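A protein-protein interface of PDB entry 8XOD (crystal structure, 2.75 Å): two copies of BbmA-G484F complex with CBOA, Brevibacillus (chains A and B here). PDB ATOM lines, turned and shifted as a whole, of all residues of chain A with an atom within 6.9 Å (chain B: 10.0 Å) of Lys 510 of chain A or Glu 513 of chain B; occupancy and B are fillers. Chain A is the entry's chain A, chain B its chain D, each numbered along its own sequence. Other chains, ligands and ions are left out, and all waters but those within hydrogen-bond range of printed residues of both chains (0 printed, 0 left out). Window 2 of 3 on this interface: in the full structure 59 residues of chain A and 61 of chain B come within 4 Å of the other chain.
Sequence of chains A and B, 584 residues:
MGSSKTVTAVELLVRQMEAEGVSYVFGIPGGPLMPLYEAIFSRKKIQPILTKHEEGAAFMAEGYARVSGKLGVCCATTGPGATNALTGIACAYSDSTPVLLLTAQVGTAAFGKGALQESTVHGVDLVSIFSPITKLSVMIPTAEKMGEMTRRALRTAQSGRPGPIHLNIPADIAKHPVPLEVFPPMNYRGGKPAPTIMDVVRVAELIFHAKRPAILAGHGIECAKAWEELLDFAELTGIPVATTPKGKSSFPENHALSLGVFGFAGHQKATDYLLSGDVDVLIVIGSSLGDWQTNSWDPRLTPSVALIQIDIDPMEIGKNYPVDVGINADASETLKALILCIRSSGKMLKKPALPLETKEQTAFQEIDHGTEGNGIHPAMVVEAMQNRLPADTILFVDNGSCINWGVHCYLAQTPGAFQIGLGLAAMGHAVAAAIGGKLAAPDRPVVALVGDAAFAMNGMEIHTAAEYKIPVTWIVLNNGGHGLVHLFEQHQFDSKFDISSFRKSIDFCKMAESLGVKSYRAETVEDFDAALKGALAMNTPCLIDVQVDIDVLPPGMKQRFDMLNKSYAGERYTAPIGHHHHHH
Among the printed residues, pairs that only touch across the chains: Lys 510 of chain A with Lys 510 of chain B, Lys 510 of chain A with Ser 514 of chain B, Met 511 of chain A with Met 460 of chain B, Ser 514 of chain A with Ile 506 of chain B, Ser 514 of chain A with Lys 510 of chain B, Ser 514 of chain A with Met 511 of chain B and Leu 515 of chain A with Ile 506 of chain B.
N of Lys 510 of chain A is in hydrogen-bond range of OD1 of Asp 507 of chain A (2.8 Å).
The backbone NH (N) of Cys 509 of chain B lies within hydrogen-bond range of the side-chain carboxylate (OD1) of Asp 507 of chain B, at 3.1 Å.
Lys 510 of chain A touches three residues of chain B.
Of chain A, only Lys 510 comes within 4 Å of Glu 513 of chain B.
No residue of chain B comes within 4 Å of Cys 509 of chain A.
No residue of chain B comes within 4 Å of Ala 512 of chain A.
Printed residues of chain A within 4 Å of Ile 506 of chain B: Ser 514 and Leu 515.
Printed residues of chain B within 4 Å of Met 511 of chain A: Met 460 and Ser 514.
Of the printed residues of chain B, Leu 515 of chain A touches Ile 506 (3.97 Å).
Ser 519 of chain B touches none of the printed residues of chain A.
The nearest residue of chain A that does not touch Glu 513 of chain B is Asp 507 of chain A (5.3 Å).
The nearest printed residue of chain B that does not touch Ser 514 of chain A is Ser 514 of chain B (5.1 Å).
Hydrophobic or aromatic side chains of chain B that line the printed part of chain A: Met 460, Ile 506 and Met 511.
Of the 13 printed residues of chain A, 6 touch a printed residue of chain B.
Along chain A the printed residues that touch a printed residue of chain B span positions 507 to 515.
Among the printed residues, 12 pairs touch across the chains.
Among the printed residues, Asp or Glu carboxylates within 4 Å of a Lys or Arg side-chain nitrogen of the other chain: Lys 510 of chain A with Glu 513 of chain B and Glu 513 of chain A with Lys 510 of chain B.
The backbone NH of Asp 507 of chain A sits at hydrogen-bond distance from the backbone carbonyl oxygen of Ser 514 of chain B, at 3.3 Å.
NZ of Lys 510 of chain A is in salt-bridge range of OE1 of Glu 513 of chain B, at 2.6 Å.
The side-chain carboxylate (OE2) of Glu 513 of chain A is in salt-bridge range of the side-chain amino group (NZ) of Lys 510 of chain B, 2.5 Å away.
O of Ser 514 of chain A is in hydrogen-bond range of N of Asp 507 of chain B, at 3.0 Å.
The backbone NH (N) of Met 511 of chain A sits close to the side-chain hydroxyl (OG) of Ser 514 of chain B (3.5 Å).
Asp 507 of chain A touches Ser 514 of chain B, and with the chains exchanged Ser 514 of chain A touches Asp 507 of chain B.
Lys 510 of chain A touches its own counterpart, Lys 510 of chain B.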
ATOM      1  N   ASP A 507     -12.591  -9.612  24.840  1.00  0.00           N
ATOM      2  CA  ASP A 507     -12.429  -8.172  24.941  1.00  0.00           C
ATOM      3  C   ASP A 507     -11.529  -7.733  23.793  1.00  0.00           C
ATOM      4  O   ASP A 507     -10.301  -7.849  23.860  1.00  0.00           O
ATOM      5  CB  ASP A 507     -11.862  -7.792  26.300  1.00  0.00           C
ATOM      6  CG  ASP A 507     -11.743  -6.284  26.480  1.00  0.00           C
ATOM      7  OD1 ASP A 507     -11.366  -5.602  25.500  1.00  0.00           O
ATOM      8  OD2 ASP A 507     -12.034  -5.779  27.596  1.00  0.00           O
ATOM      9  N   PHE A 508     -12.156  -7.243  22.726  1.00  0.00           N
ATOM     10  CA  PHE A 508     -11.412  -6.856  21.539  1.00  0.00           C
ATOM     11  C   PHE A 508     -10.722  -5.504  21.665  1.00  0.00           C
ATOM     12  O   PHE A 508      -9.823  -5.232  20.861  1.00  0.00           O
ATOM     13  CB  PHE A 508     -12.332  -6.888  20.315  1.00  0.00           C
ATOM     14  CG  PHE A 508     -12.847  -8.257  20.011  1.00  0.00           C
ATOM     15  CD1 PHE A 508     -12.042  -9.191  19.380  1.00  0.00           C
ATOM     16  CD2 PHE A 508     -14.119  -8.633  20.403  1.00  0.00           C
ATOM     17  CE1 PHE A 508     -12.512 -10.454  19.117  1.00  0.00           C
ATOM     18  CE2 PHE A 508     -14.593  -9.901  20.145  1.00  0.00           C
ATOM     19  CZ  PHE A 508     -13.789 -10.811  19.500  1.00  0.00           C
ATOM     20  N   CYS A 509     -11.046  -4.671  22.669  1.00  0.00           N
ATOM     21  CA  CYS A 509     -10.252  -3.454  22.793  1.00  0.00           C
ATOM     22  C   CYS A 509      -8.932  -3.726  23.492  1.00  0.00           C
ATOM     23  O   CYS A 509      -7.893  -3.182  23.111  1.00  0.00           O
ATOM     24  CB  CYS A 509     -10.994  -2.365  23.572  1.00  0.00           C
ATOM     25  SG  CYS A 509     -12.749  -2.184  23.247  1.00  0.00           S
ATOM     26  N   LYS A 510      -8.931  -4.633  24.453  1.00  0.00           N
ATOM     27  CA  LYS A 510      -7.667  -5.097  24.998  1.00  0.00           C
ATOM     28  C   LYS A 510      -6.883  -5.857  23.946  1.00  0.00           C
ATOM     29  O   LYS A 510      -5.660  -5.712  23.848  1.00  0.00           O
ATOM     30  CB  LYS A 510      -7.928  -5.924  26.257  1.00  0.00           C
ATOM     31  CG  LYS A 510      -8.575  -5.046  27.310  1.00  0.00           C
ATOM     32  CD  LYS A 510      -8.892  -5.796  28.568  1.00  0.00           C
ATOM     33  CE  LYS A 510      -8.555  -4.960  29.786  1.00  0.00           C
ATOM     34  NZ  LYS A 510      -8.906  -5.711  31.002  1.00  0.00           N
ATOM     35  N   MET A 511      -7.567  -6.632  23.114  1.00  0.00           N
ATOM     36  CA  MET A 511      -6.832  -7.309  22.061  1.00  0.00           C
ATOM     37  C   MET A 511      -6.240  -6.300  21.092  1.00  0.00           C
ATOM     38  O   MET A 511      -5.087  -6.425  20.676  1.00  0.00           O
ATOM     39  CB  MET A 511      -7.728  -8.312  21.339  1.00  0.00           C
ATOM     40  CG  MET A 511      -6.958  -9.293  20.457  1.00  0.00           C
ATOM     41  SD  MET A 511      -8.087 -10.259  19.447  1.00  0.00           S
ATOM     42  CE  MET A 511      -7.004 -10.940  18.178  1.00  0.00           C
ATOM     43  N   ALA A 512      -6.998  -5.260  20.752  1.00  0.00           N
ATOM     44  CA  ALA A 512      -6.461  -4.233  19.867  1.00  0.00           C
ATOM     45  C   ALA A 512      -5.248  -3.542  20.482  1.00  0.00           C
ATOM     46  O   ALA A 512      -4.243  -3.307  19.797  1.00  0.00           O
ATOM     47  CB  ALA A 512      -7.546  -3.215  19.521  1.00  0.00           C
ATOM     48  N   GLU A 513      -5.376  -3.215  21.741  1.00  0.00           N
ATOM     49  CA  GLU A 513      -4.349  -2.487  22.391  1.00  0.00           C
ATOM     50  C   GLU A 513      -3.065  -3.170  22.477  1.00  0.00           C
ATOM     51  O   GLU A 513      -2.040  -2.564  22.350  1.00  0.00           O
ATOM     52  CB  GLU A 513      -4.750  -2.132  23.769  1.00  0.00           C
ATOM     53  CG  GLU A 513      -3.786  -1.137  24.319  1.00  0.00           C
ATOM     54  CD  GLU A 513      -3.832  -1.078  25.797  1.00  0.00           C
ATOM     55  OE1 GLU A 513      -2.746  -0.952  26.372  1.00  0.00           O
ATOM     56  OE2 GLU A 513      -4.942  -1.156  26.353  1.00  0.00           O
ATOM     57  N   SER A 514      -3.088  -4.476  22.610  1.00  0.00           N
ATOM     58  CA  SER A 514      -1.861  -5.231  22.723  1.00  0.00           C
ATOM     59  C   SER A 514      -1.140  -5.434  21.435  1.00  0.00           C
ATOM     60  O   SER A 514      -0.018  -5.846  21.431  1.00  0.00           O
ATOM     61  CB  SER A 514      -2.134  -6.560  23.371  1.00  0.00           C
ATOM     62  OG  SER A 514      -2.419  -7.521  22.404  1.00  0.00           O
ATOM     63  N   LEU A 515      -1.825  -5.104  20.369  1.00  0.00           N
ATOM     64  CA  LEU A 515      -1.286  -5.263  19.059  1.00  0.00           C
ATOM     65  C   LEU A 515      -0.949  -3.938  18.503  1.00  0.00           C
ATOM     66  O   LEU A 515      -0.445  -3.850  17.423  1.00  0.00           O
ATOM     67  CB  LEU A 515      -2.314  -5.923  18.190  1.00  0.00           C
ATOM     68  CG  LEU A 515      -2.553  -7.342  18.639  1.00  0.00           C
ATOM     69  CD1 LEU A 515      -3.843  -7.845  18.077  1.00  0.00           C
ATOM     70  CD2 LEU A 515      -1.443  -8.168  18.077  1.00  0.00           C
ATOM     71  N   SER A 519      -8.563   1.634  19.840  1.00  0.00           N
ATOM     72  CA  SER A 519      -9.822   0.997  19.902  1.00  0.00           C
ATOM     73  C   SER A 519     -10.814   1.758  20.707  1.00  0.00           C
ATOM     74  O   SER A 519     -10.471   2.628  21.448  1.00  0.00           O
ATOM     75  CB  SER A 519      -9.628  -0.342  20.562  1.00  0.00           C
ATOM     76  OG  SER A 519      -8.924  -0.198  21.755  1.00  0.00           O
ATOM     77  N   ARG A 521     -14.870   1.015  22.641  1.00  0.00           N
ATOM     78  CA  ARG A 521     -15.915   0.064  23.002  1.00  0.00           C
ATOM     79  C   ARG A 521     -17.230   0.818  22.869  1.00  0.00           C
ATOM     80  O   ARG A 521     -17.264   2.029  23.091  1.00  0.00           O
ATOM     81  CB  ARG A 521     -15.724  -0.431  24.434  1.00  0.00           C
ATOM     82  CG  ARG A 521     -16.758  -1.452  24.882  1.00  0.00           C
ATOM     83  CD  ARG A 521     -16.124  -2.550  25.721  1.00  0.00           C
ATOM     84  NE  ARG A 521     -14.865  -3.018  25.147  1.00  0.00           N
ATOM     85  CZ  ARG A 521     -14.560  -4.296  24.959  1.00  0.00           C
ATOM     86  NH1 ARG A 521     -15.423  -5.244  25.298  1.00  0.00           N
ATOM     87  NH2 ARG A 521     -13.391  -4.631  24.430  1.00  0.00           N
ATOM     88  N   LEU A 543     -10.270  -0.184  15.803  1.00  0.00           N
ATOM     89  CA  LEU A 543     -11.231  -1.242  16.069  1.00  0.00           C
ATOM     90  C   LEU A 543     -12.304  -0.699  17.001  1.00  0.00           C
ATOM     91  O   LEU A 543     -12.006   0.030  17.947  1.00  0.00           O
ATOM     92  CB  LEU A 543     -10.523  -2.470  16.664  1.00  0.00           C
ATOM     93  CG  LEU A 543     -11.373  -3.654  17.093  1.00  0.00           C
ATOM     94  CD1 LEU A 543     -10.639  -4.977  16.756  1.00  0.00           C
ATOM     95  CD2 LEU A 543     -11.704  -3.511  18.591  1.00  0.00           C
ATOM     96  N   ASP A 545     -15.459  -2.108  19.249  1.00  0.00           N
ATOM     97  CA  ASP A 545     -16.032  -3.338  19.778  1.00  0.00           C
ATOM     98  C   ASP A 545     -17.467  -3.042  20.203  1.00  0.00           C
ATOM     99  O   ASP A 545     -17.697  -2.344  21.195  1.00  0.00           O
ATOM    100  CB  ASP A 545     -15.189  -3.871  20.940  1.00  0.00           C
ATOM    101  CG  ASP A 545     -15.605  -5.289  21.391  1.00  0.00           C
ATOM    102  OD1 ASP A 545     -16.813  -5.614  21.366  1.00  0.00           O
ATOM    103  OD2 ASP A 545     -14.716  -6.078  21.789  1.00  0.00           O
ATOM    104  N   PHE B 455       2.935 -17.680  18.289  1.00  0.00           N
ATOM    105  CA  PHE B 455       1.782 -17.412  19.140  1.00  0.00           C
ATOM    106  C   PHE B 455       0.760 -16.554  18.407  1.00  0.00           C
ATOM    107  O   PHE B 455      -0.451 -16.750  18.564  1.00  0.00           O
ATOM    108  CB  PHE B 455       2.199 -16.747  20.472  1.00  0.00           C
ATOM    109  CG  PHE B 455       1.108 -16.805  21.523  1.00  0.00           C
ATOM    110  CD1 PHE B 455       0.017 -15.954  21.461  1.00  0.00           C
ATOM    111  CD2 PHE B 455       1.127 -17.768  22.519  1.00  0.00           C
ATOM    112  CE1 PHE B 455      -1.024 -16.043  22.379  1.00  0.00           C
ATOM    113  CE2 PHE B 455       0.092 -17.841  23.457  1.00  0.00           C
ATOM    114  CZ  PHE B 455      -0.985 -16.974  23.374  1.00  0.00           C
ATOM    115  N   GLY B 459      -2.225 -18.427  18.852  1.00  0.00           N
ATOM    116  CA  GLY B 459      -2.373 -18.031  20.235  1.00  0.00           C
ATOM    117  C   GLY B 459      -3.798 -17.740  20.646  1.00  0.00           C
ATOM    118  O   GLY B 459      -4.072 -17.570  21.846  1.00  0.00           O
ATOM    119  N   MET B 460      -4.699 -17.579  19.680  1.00  0.00           N
ATOM    120  CA  MET B 460      -6.080 -17.308  20.049  1.00  0.00           C
ATOM    121  C   MET B 460      -6.711 -18.487  20.773  1.00  0.00           C
ATOM    122  O   MET B 460      -7.683 -18.303  21.518  1.00  0.00           O
ATOM    123  CB  MET B 460      -6.888 -16.930  18.798  1.00  0.00           C
ATOM    124  CG  MET B 460      -6.433 -15.614  18.168  1.00  0.00           C
ATOM    125  SD  MET B 460      -6.643 -14.119  19.194  1.00  0.00           S
ATOM    126  CE  MET B 460      -8.400 -14.206  19.562  1.00  0.00           C
ATOM    127  N   ILE B 462      -5.686 -19.895  23.400  1.00  0.00           N
ATOM    128  CA  ILE B 462      -5.654 -19.832  24.857  1.00  0.00           C
ATOM    129  C   ILE B 462      -7.002 -19.398  25.391  1.00  0.00           C
ATOM    130  O   ILE B 462      -7.296 -19.632  26.570  1.00  0.00           O
ATOM    131  CB  ILE B 462      -4.584 -18.880  25.436  1.00  0.00           C
ATOM    132  CG1 ILE B 462      -4.762 -17.466  24.897  1.00  0.00           C
ATOM    133  CG2 ILE B 462      -3.174 -19.390  25.200  1.00  0.00           C
ATOM    134  CD1 ILE B 462      -4.029 -16.439  25.723  1.00  0.00           C
ATOM    135  N   HIS B 463      -7.826 -18.748  24.563  1.00  0.00           N
ATOM    136  CA  HIS B 463      -9.187 -18.446  24.988  1.00  0.00           C
ATOM    137  C   HIS B 463     -10.001 -19.709  25.212  1.00  0.00           C
ATOM    138  O   HIS B 463     -10.860 -19.750  26.102  1.00  0.00           O
ATOM    139  CB  HIS B 463      -9.886 -17.567  23.969  1.00  0.00           C
ATOM    140  CG  HIS B 463     -11.266 -17.170  24.389  1.00  0.00           C
ATOM    141  ND1 HIS B 463     -12.399 -17.789  23.906  1.00  0.00           N
ATOM    142  CD2 HIS B 463     -11.695 -16.229  25.267  1.00  0.00           C
ATOM    143  CE1 HIS B 463     -13.467 -17.239  24.458  1.00  0.00           C
ATOM    144  NE2 HIS B 463     -13.067 -16.291  25.289  1.00  0.00           N
ATOM    145  N   ALA B 466      -9.102 -21.216  28.364  1.00  0.00           N
ATOM    146  CA  ALA B 466      -9.775 -20.382  29.351  1.00  0.00           C
ATOM    147  C   ALA B 466     -11.241 -20.761  29.510  1.00  0.00           C
ATOM    148  O   ALA B 466     -11.762 -20.819  30.630  1.00  0.00           O
ATOM    149  CB  ALA B 466      -9.663 -18.916  28.928  1.00  0.00           C
ATOM    150  N   ILE B 506       4.567  -7.499  20.154  1.00  0.00           N
ATOM    151  CA  ILE B 506       3.225  -7.748  20.670  1.00  0.00           C
ATOM    152  C   ILE B 506       3.252  -7.776  22.195  1.00  0.00           C
ATOM    153  O   ILE B 506       4.234  -8.206  22.816  1.00  0.00           O
ATOM    154  CB  ILE B 506       2.667  -9.059  20.081  1.00  0.00           C
ATOM    155  CG1 ILE B 506       2.433  -8.896  18.566  1.00  0.00           C
ATOM    156  CG2 ILE B 506       1.388  -9.488  20.803  1.00  0.00           C
ATOM    157  CD1 ILE B 506       2.272 -10.181  17.812  1.00  0.00           C
ATOM    158  N   ASP B 507       2.162  -7.315  22.816  1.00  0.00           N
ATOM    159  CA  ASP B 507       2.029  -7.347  24.278  1.00  0.00           C
ATOM    160  C   ASP B 507       1.215  -8.588  24.647  1.00  0.00           C
ATOM    161  O   ASP B 507      -0.015  -8.545  24.738  1.00  0.00           O
ATOM    162  CB  ASP B 507       1.372  -6.066  24.788  1.00  0.00           C
ATOM    163  CG  ASP B 507       1.235  -6.039  26.306  1.00  0.00           C
ATOM    164  OD1 ASP B 507       1.369  -7.109  26.939  1.00  0.00           O
ATOM    165  OD2 ASP B 507       0.997  -4.946  26.873  1.00  0.00           O
ATOM    166  N   PHE B 508       1.918  -9.686  24.953  1.00  0.00           N
ATOM    167  CA  PHE B 508       1.223 -10.942  25.193  1.00  0.00           C
ATOM    168  C   PHE B 508       0.541 -10.999  26.551  1.00  0.00           C
ATOM    169  O   PHE B 508      -0.344 -11.839  26.743  1.00  0.00           O
ATOM    170  CB  PHE B 508       2.192 -12.125  24.998  1.00  0.00           C
ATOM    171  CG  PHE B 508       2.578 -12.337  23.552  1.00  0.00           C
ATOM    172  CD1 PHE B 508       1.712 -12.962  22.675  1.00  0.00           C
ATOM    173  CD2 PHE B 508       3.782 -11.862  23.059  1.00  0.00           C
ATOM    174  CE1 PHE B 508       2.042 -13.116  21.340  1.00  0.00           C
ATOM    175  CE2 PHE B 508       4.120 -12.025  21.724  1.00  0.00           C
ATOM    176  CZ  PHE B 508       3.247 -12.650  20.865  1.00  0.00           C
ATOM    177  N   CYS B 509       0.853 -10.090  27.468  1.00  0.00           N
ATOM    178  CA  CYS B 509       0.115 -10.101  28.719  1.00  0.00           C
ATOM    179  C   CYS B 509      -1.212  -9.367  28.601  1.00  0.00           C
ATOM    180  O   CYS B 509      -2.220  -9.836  29.133  1.00  0.00           O
ATOM    181  CB  CYS B 509       0.938  -9.448  29.821  1.00  0.00           C
ATOM    182  SG  CYS B 509       2.419 -10.325  30.265  1.00  0.00           S
ATOM    183  N   LYS B 510      -1.253  -8.270  27.832  1.00  0.00           N
ATOM    184  CA  LYS B 510      -2.525  -7.634  27.497  1.00  0.00           C
ATOM    185  C   LYS B 510      -3.380  -8.572  26.674  1.00  0.00           C
ATOM    186  O   LYS B 510      -4.597  -8.633  26.867  1.00  0.00           O
ATOM    187  CB  LYS B 510      -2.302  -6.305  26.741  1.00  0.00           C
ATOM    188  CG  LYS B 510      -3.465  -5.273  26.828  1.00  0.00           C
ATOM    189  CD  LYS B 510      -3.337  -4.478  28.122  1.00  0.00           C
ATOM    190  CE  LYS B 510      -4.626  -3.796  28.562  1.00  0.00           C
ATOM    191  NZ  LYS B 510      -4.561  -2.324  28.479  1.00  0.00           N
ATOM    192  N   MET B 511      -2.752  -9.333  25.771  1.00  0.00           N
ATOM    193  CA  MET B 511      -3.514 -10.279  24.965  1.00  0.00           C
ATOM    194  C   MET B 511      -4.120 -11.387  25.811  1.00  0.00           C
ATOM    195  O   MET B 511      -5.286 -11.747  25.611  1.00  0.00           O
ATOM    196  CB  MET B 511      -2.646 -10.881  23.869  1.00  0.00           C
ATOM    197  CG  MET B 511      -3.498 -11.494  22.764  1.00  0.00           C
ATOM    198  SD  MET B 511      -2.473 -12.151  21.452  1.00  0.00           S
ATOM    199  CE  MET B 511      -1.245 -12.981  22.442  1.00  0.00           C
ATOM    200  N   ALA B 512      -3.359 -11.934  26.770  1.00  0.00           N
ATOM    201  CA  ALA B 512      -3.925 -12.948  27.654  1.00  0.00           C
ATOM    202  C   ALA B 512      -5.107 -12.349  28.392  1.00  0.00           C
ATOM    203  O   ALA B 512      -6.163 -12.975  28.535  1.00  0.00           O
ATOM    204  CB  ALA B 512      -2.869 -13.478  28.624  1.00  0.00           C
ATOM    205  N   GLU B 513      -4.958 -11.100  28.811  1.00  0.00           N
ATOM    206  CA  GLU B 513      -6.054 -10.404  29.467  1.00  0.00           C
ATOM    207  C   GLU B 513      -7.301 -10.322  28.579  1.00  0.00           C
ATOM    208  O   GLU B 513      -8.396 -10.703  28.991  1.00  0.00           O
ATOM    209  CB  GLU B 513      -5.564  -9.007  29.849  1.00  0.00           C
ATOM    210  CG  GLU B 513      -6.296  -8.239  30.955  1.00  0.00           C
ATOM    211  CD  GLU B 513      -5.680  -6.850  31.223  1.00  0.00           C
ATOM    212  OE1 GLU B 513      -6.416  -5.973  31.714  1.00  0.00           O
ATOM    213  OE2 GLU B 513      -4.474  -6.629  30.953  1.00  0.00           O
ATOM    214  N   SER B 514      -7.179  -9.853  27.350  1.00  0.00           N
ATOM    215  CA  SER B 514      -8.324  -9.947  26.430  1.00  0.00           C
ATOM    216  C   SER B 514      -8.957 -11.354  26.378  1.00  0.00           C
ATOM    217  O   SER B 514     -10.188 -11.483  26.218  1.00  0.00           O
ATOM    218  CB  SER B 514      -7.915  -9.300  25.090  1.00  0.00           C
ATOM    219  OG  SER B 514      -6.551  -9.514  24.727  1.00  0.00           O
ATOM    220  N   LEU B 515      -8.176 -12.427  26.531  1.00  0.00           N
ATOM    221  CA  LEU B 515      -8.790 -13.726  26.362  1.00  0.00           C
ATOM    222  C   LEU B 515      -9.159 -14.355  27.690  1.00  0.00           C
ATOM    223  O   LEU B 515      -9.675 -15.473  27.693  1.00  0.00           O
ATOM    224  CB  LEU B 515      -7.907 -14.640  25.547  1.00  0.00           C
ATOM    225  CG  LEU B 515      -7.462 -13.935  24.275  1.00  0.00           C
ATOM    226  CD1 LEU B 515      -6.162 -14.528  23.800  1.00  0.00           C
ATOM    227  CD2 LEU B 515      -8.547 -13.962  23.190  1.00  0.00           C
ATOM    228  N   GLY B 516      -8.992 -13.636  28.802  1.00  0.00           N
ATOM    229  CA  GLY B 516      -9.397 -14.159  30.096  1.00  0.00           C
ATOM    230  C   GLY B 516      -8.392 -15.106  30.709  1.00  0.00           C
ATOM    231  O   GLY B 516      -8.783 -16.008  31.445  1.00  0.00           O
ATOM    232  N   VAL B 517      -7.101 -14.910  30.436  1.00  0.00           N
ATOM    233  CA  VAL B 517      -6.029 -15.780  30.895  1.00  0.00           C
ATOM    234  C   VAL B 517      -5.068 -14.973  31.761  1.00  0.00           C
ATOM    235  O   VAL B 517      -4.649 -13.868  31.382  1.00  0.00           O
ATOM    236  CB  VAL B 517      -5.290 -16.420  29.704  1.00  0.00           C
ATOM    237  CG1 VAL B 517      -4.303 -17.496  30.142  1.00  0.00           C
ATOM    238  CG2 VAL B 517      -6.296 -17.024  28.750  1.00  0.00           C
ATOM    239  N   LYS B 518      -4.711 -15.535  32.917  1.00  0.00           N
ATOM    240  CA  LYS B 518      -3.786 -14.881  33.833  1.00  0.00           C
ATOM    241  C   LYS B 518      -2.370 -14.871  33.245  1.00  0.00           C
ATOM    242  O   LYS B 518      -1.958 -15.795  32.554  1.00  0.00           O
ATOM    243  CB  LYS B 518      -3.795 -15.583  35.196  1.00  0.00           C
ATOM    244  CG  LYS B 518      -3.044 -14.831  36.287  1.00  0.00           C
ATOM    245  CD  LYS B 518      -3.916 -13.813  37.017  1.00  0.00           C
ATOM    246  CE  LYS B 518      -3.070 -12.959  37.941  1.00  0.00           C
ATOM    247  NZ  LYS B 518      -2.818 -11.629  37.341  1.00  0.00           N
ATOM    248  N   SER B 519      -1.641 -13.800  33.531  1.00  0.00           N
ATOM    249  CA  SER B 519      -0.462 -13.415  32.779  1.00  0.00           C
ATOM    250  C   SER B 519       0.665 -12.987  33.717  1.00  0.00           C
ATOM    251  O   SER B 519       0.429 -12.526  34.840  1.00  0.00           O
ATOM    252  CB  SER B 519      -0.812 -12.264  31.817  1.00  0.00           C
ATOM    253  OG  SER B 519       0.285 -11.977  30.972  1.00  0.00           O
ATOM    254  N   TYR B 520       1.902 -13.188  33.251  1.00  0.00           N
ATOM    255  CA  TYR B 520       3.112 -12.712  33.913  1.00  0.00           C
ATOM    256  C   TYR B 520       4.059 -12.133  32.876  1.00  0.00           C
ATOM    257  O   TYR B 520       4.194 -12.684  31.780  1.00  0.00           O
ATOM    258  CB  TYR B 520       3.842 -13.839  34.643  1.00  0.00           C
ATOM    259  CG  TYR B 520       3.206 -14.295  35.926  1.00  0.00           C
ATOM    260  CD1 TYR B 520       3.060 -13.413  36.980  1.00  0.00           C
ATOM    261  CD2 TYR B 520       2.801 -15.619  36.106  1.00  0.00           C
ATOM    262  CE1 TYR B 520       2.502 -13.806  38.163  1.00  0.00           C
ATOM    263  CE2 TYR B 520       2.249 -16.031  37.295  1.00  0.00           C
ATOM    264  CZ  TYR B 520       2.104 -15.123  38.321  1.00  0.00           C
ATOM    265  OH  TYR B 520       1.552 -15.508  39.519  1.00  0.00           O
ATOM    266  N   ARG B 521       4.721 -11.038  33.219  1.00  0.00           N
ATOM    267  CA  ARG B 521       5.815 -10.521  32.408  1.00  0.00           C
ATOM    268  C   ARG B 521       7.138 -10.742  33.135  1.00  0.00           C
ATOM    269  O   ARG B 521       7.229 -10.565  34.355  1.00  0.00           O
ATOM    270  CB  ARG B 521       5.610  -9.030  32.094  1.00  0.00           C
ATOM    271  CG  ARG B 521       6.498  -8.473  30.975  1.00  0.00           C
ATOM    272  CD  ARG B 521       6.531  -6.920  30.961  1.00  0.00           C
ATOM    273  NE  ARG B 521       5.231  -6.295  31.216  1.00  0.00           N
ATOM    274  CZ  ARG B 521       4.209  -6.345  30.368  1.00  0.00           C
ATOM    275  NH1 ARG B 521       4.349  -6.993  29.221  1.00  0.00           N
ATOM    276  NH2 ARG B 521       3.054  -5.759  30.665  1.00  0.00           N
ATOM    277  N   PRO B 541      -5.312 -21.767  33.245  1.00  0.00           N
ATOM    278  CA  PRO B 541      -4.349 -21.407  32.192  1.00  0.00           C
ATOM    279  C   PRO B 541      -3.511 -20.204  32.603  1.00  0.00           C
ATOM    280  O   PRO B 541      -3.969 -19.333  33.346  1.00  0.00           O
ATOM    281  CB  PRO B 541      -5.234 -21.079  30.979  1.00  0.00           C
ATOM    282  CG  PRO B 541      -6.597 -21.554  31.327  1.00  0.00           C
ATOM    283  CD  PRO B 541      -6.711 -21.659  32.806  1.00  0.00           C
ATOM    284  N   CYS B 542      -2.296 -20.127  32.058  1.00  0.00           N
ATOM    285  CA  CYS B 542      -1.428 -18.994  32.341  1.00  0.00           C
ATOM    286  C   CYS B 542      -0.412 -18.794  31.220  1.00  0.00           C
ATOM    287  O   CYS B 542       0.004 -19.752  30.562  1.00  0.00           O
ATOM    288  CB  CYS B 542      -0.705 -19.207  33.679  1.00  0.00           C
ATOM    289  SG  CYS B 542       0.683 -18.098  33.973  1.00  0.00           S
ATOM    290  N   LEU B 543       0.001 -17.535  31.028  1.00  0.00           N
ATOM    291  CA  LEU B 543       0.944 -17.179  29.978  1.00  0.00           C
ATOM    292  C   LEU B 543       2.085 -16.356  30.559  1.00  0.00           C
ATOM    293  O   LEU B 543       1.864 -15.474  31.397  1.00  0.00           O
ATOM    294  CB  LEU B 543       0.246 -16.425  28.858  1.00  0.00           C
ATOM    295  CG  LEU B 543       1.123 -16.087  27.662  1.00  0.00           C
ATOM    296  CD1 LEU B 543       0.372 -16.353  26.361  1.00  0.00           C
ATOM    297  CD2 LEU B 543       1.569 -14.629  27.771  1.00  0.00           C
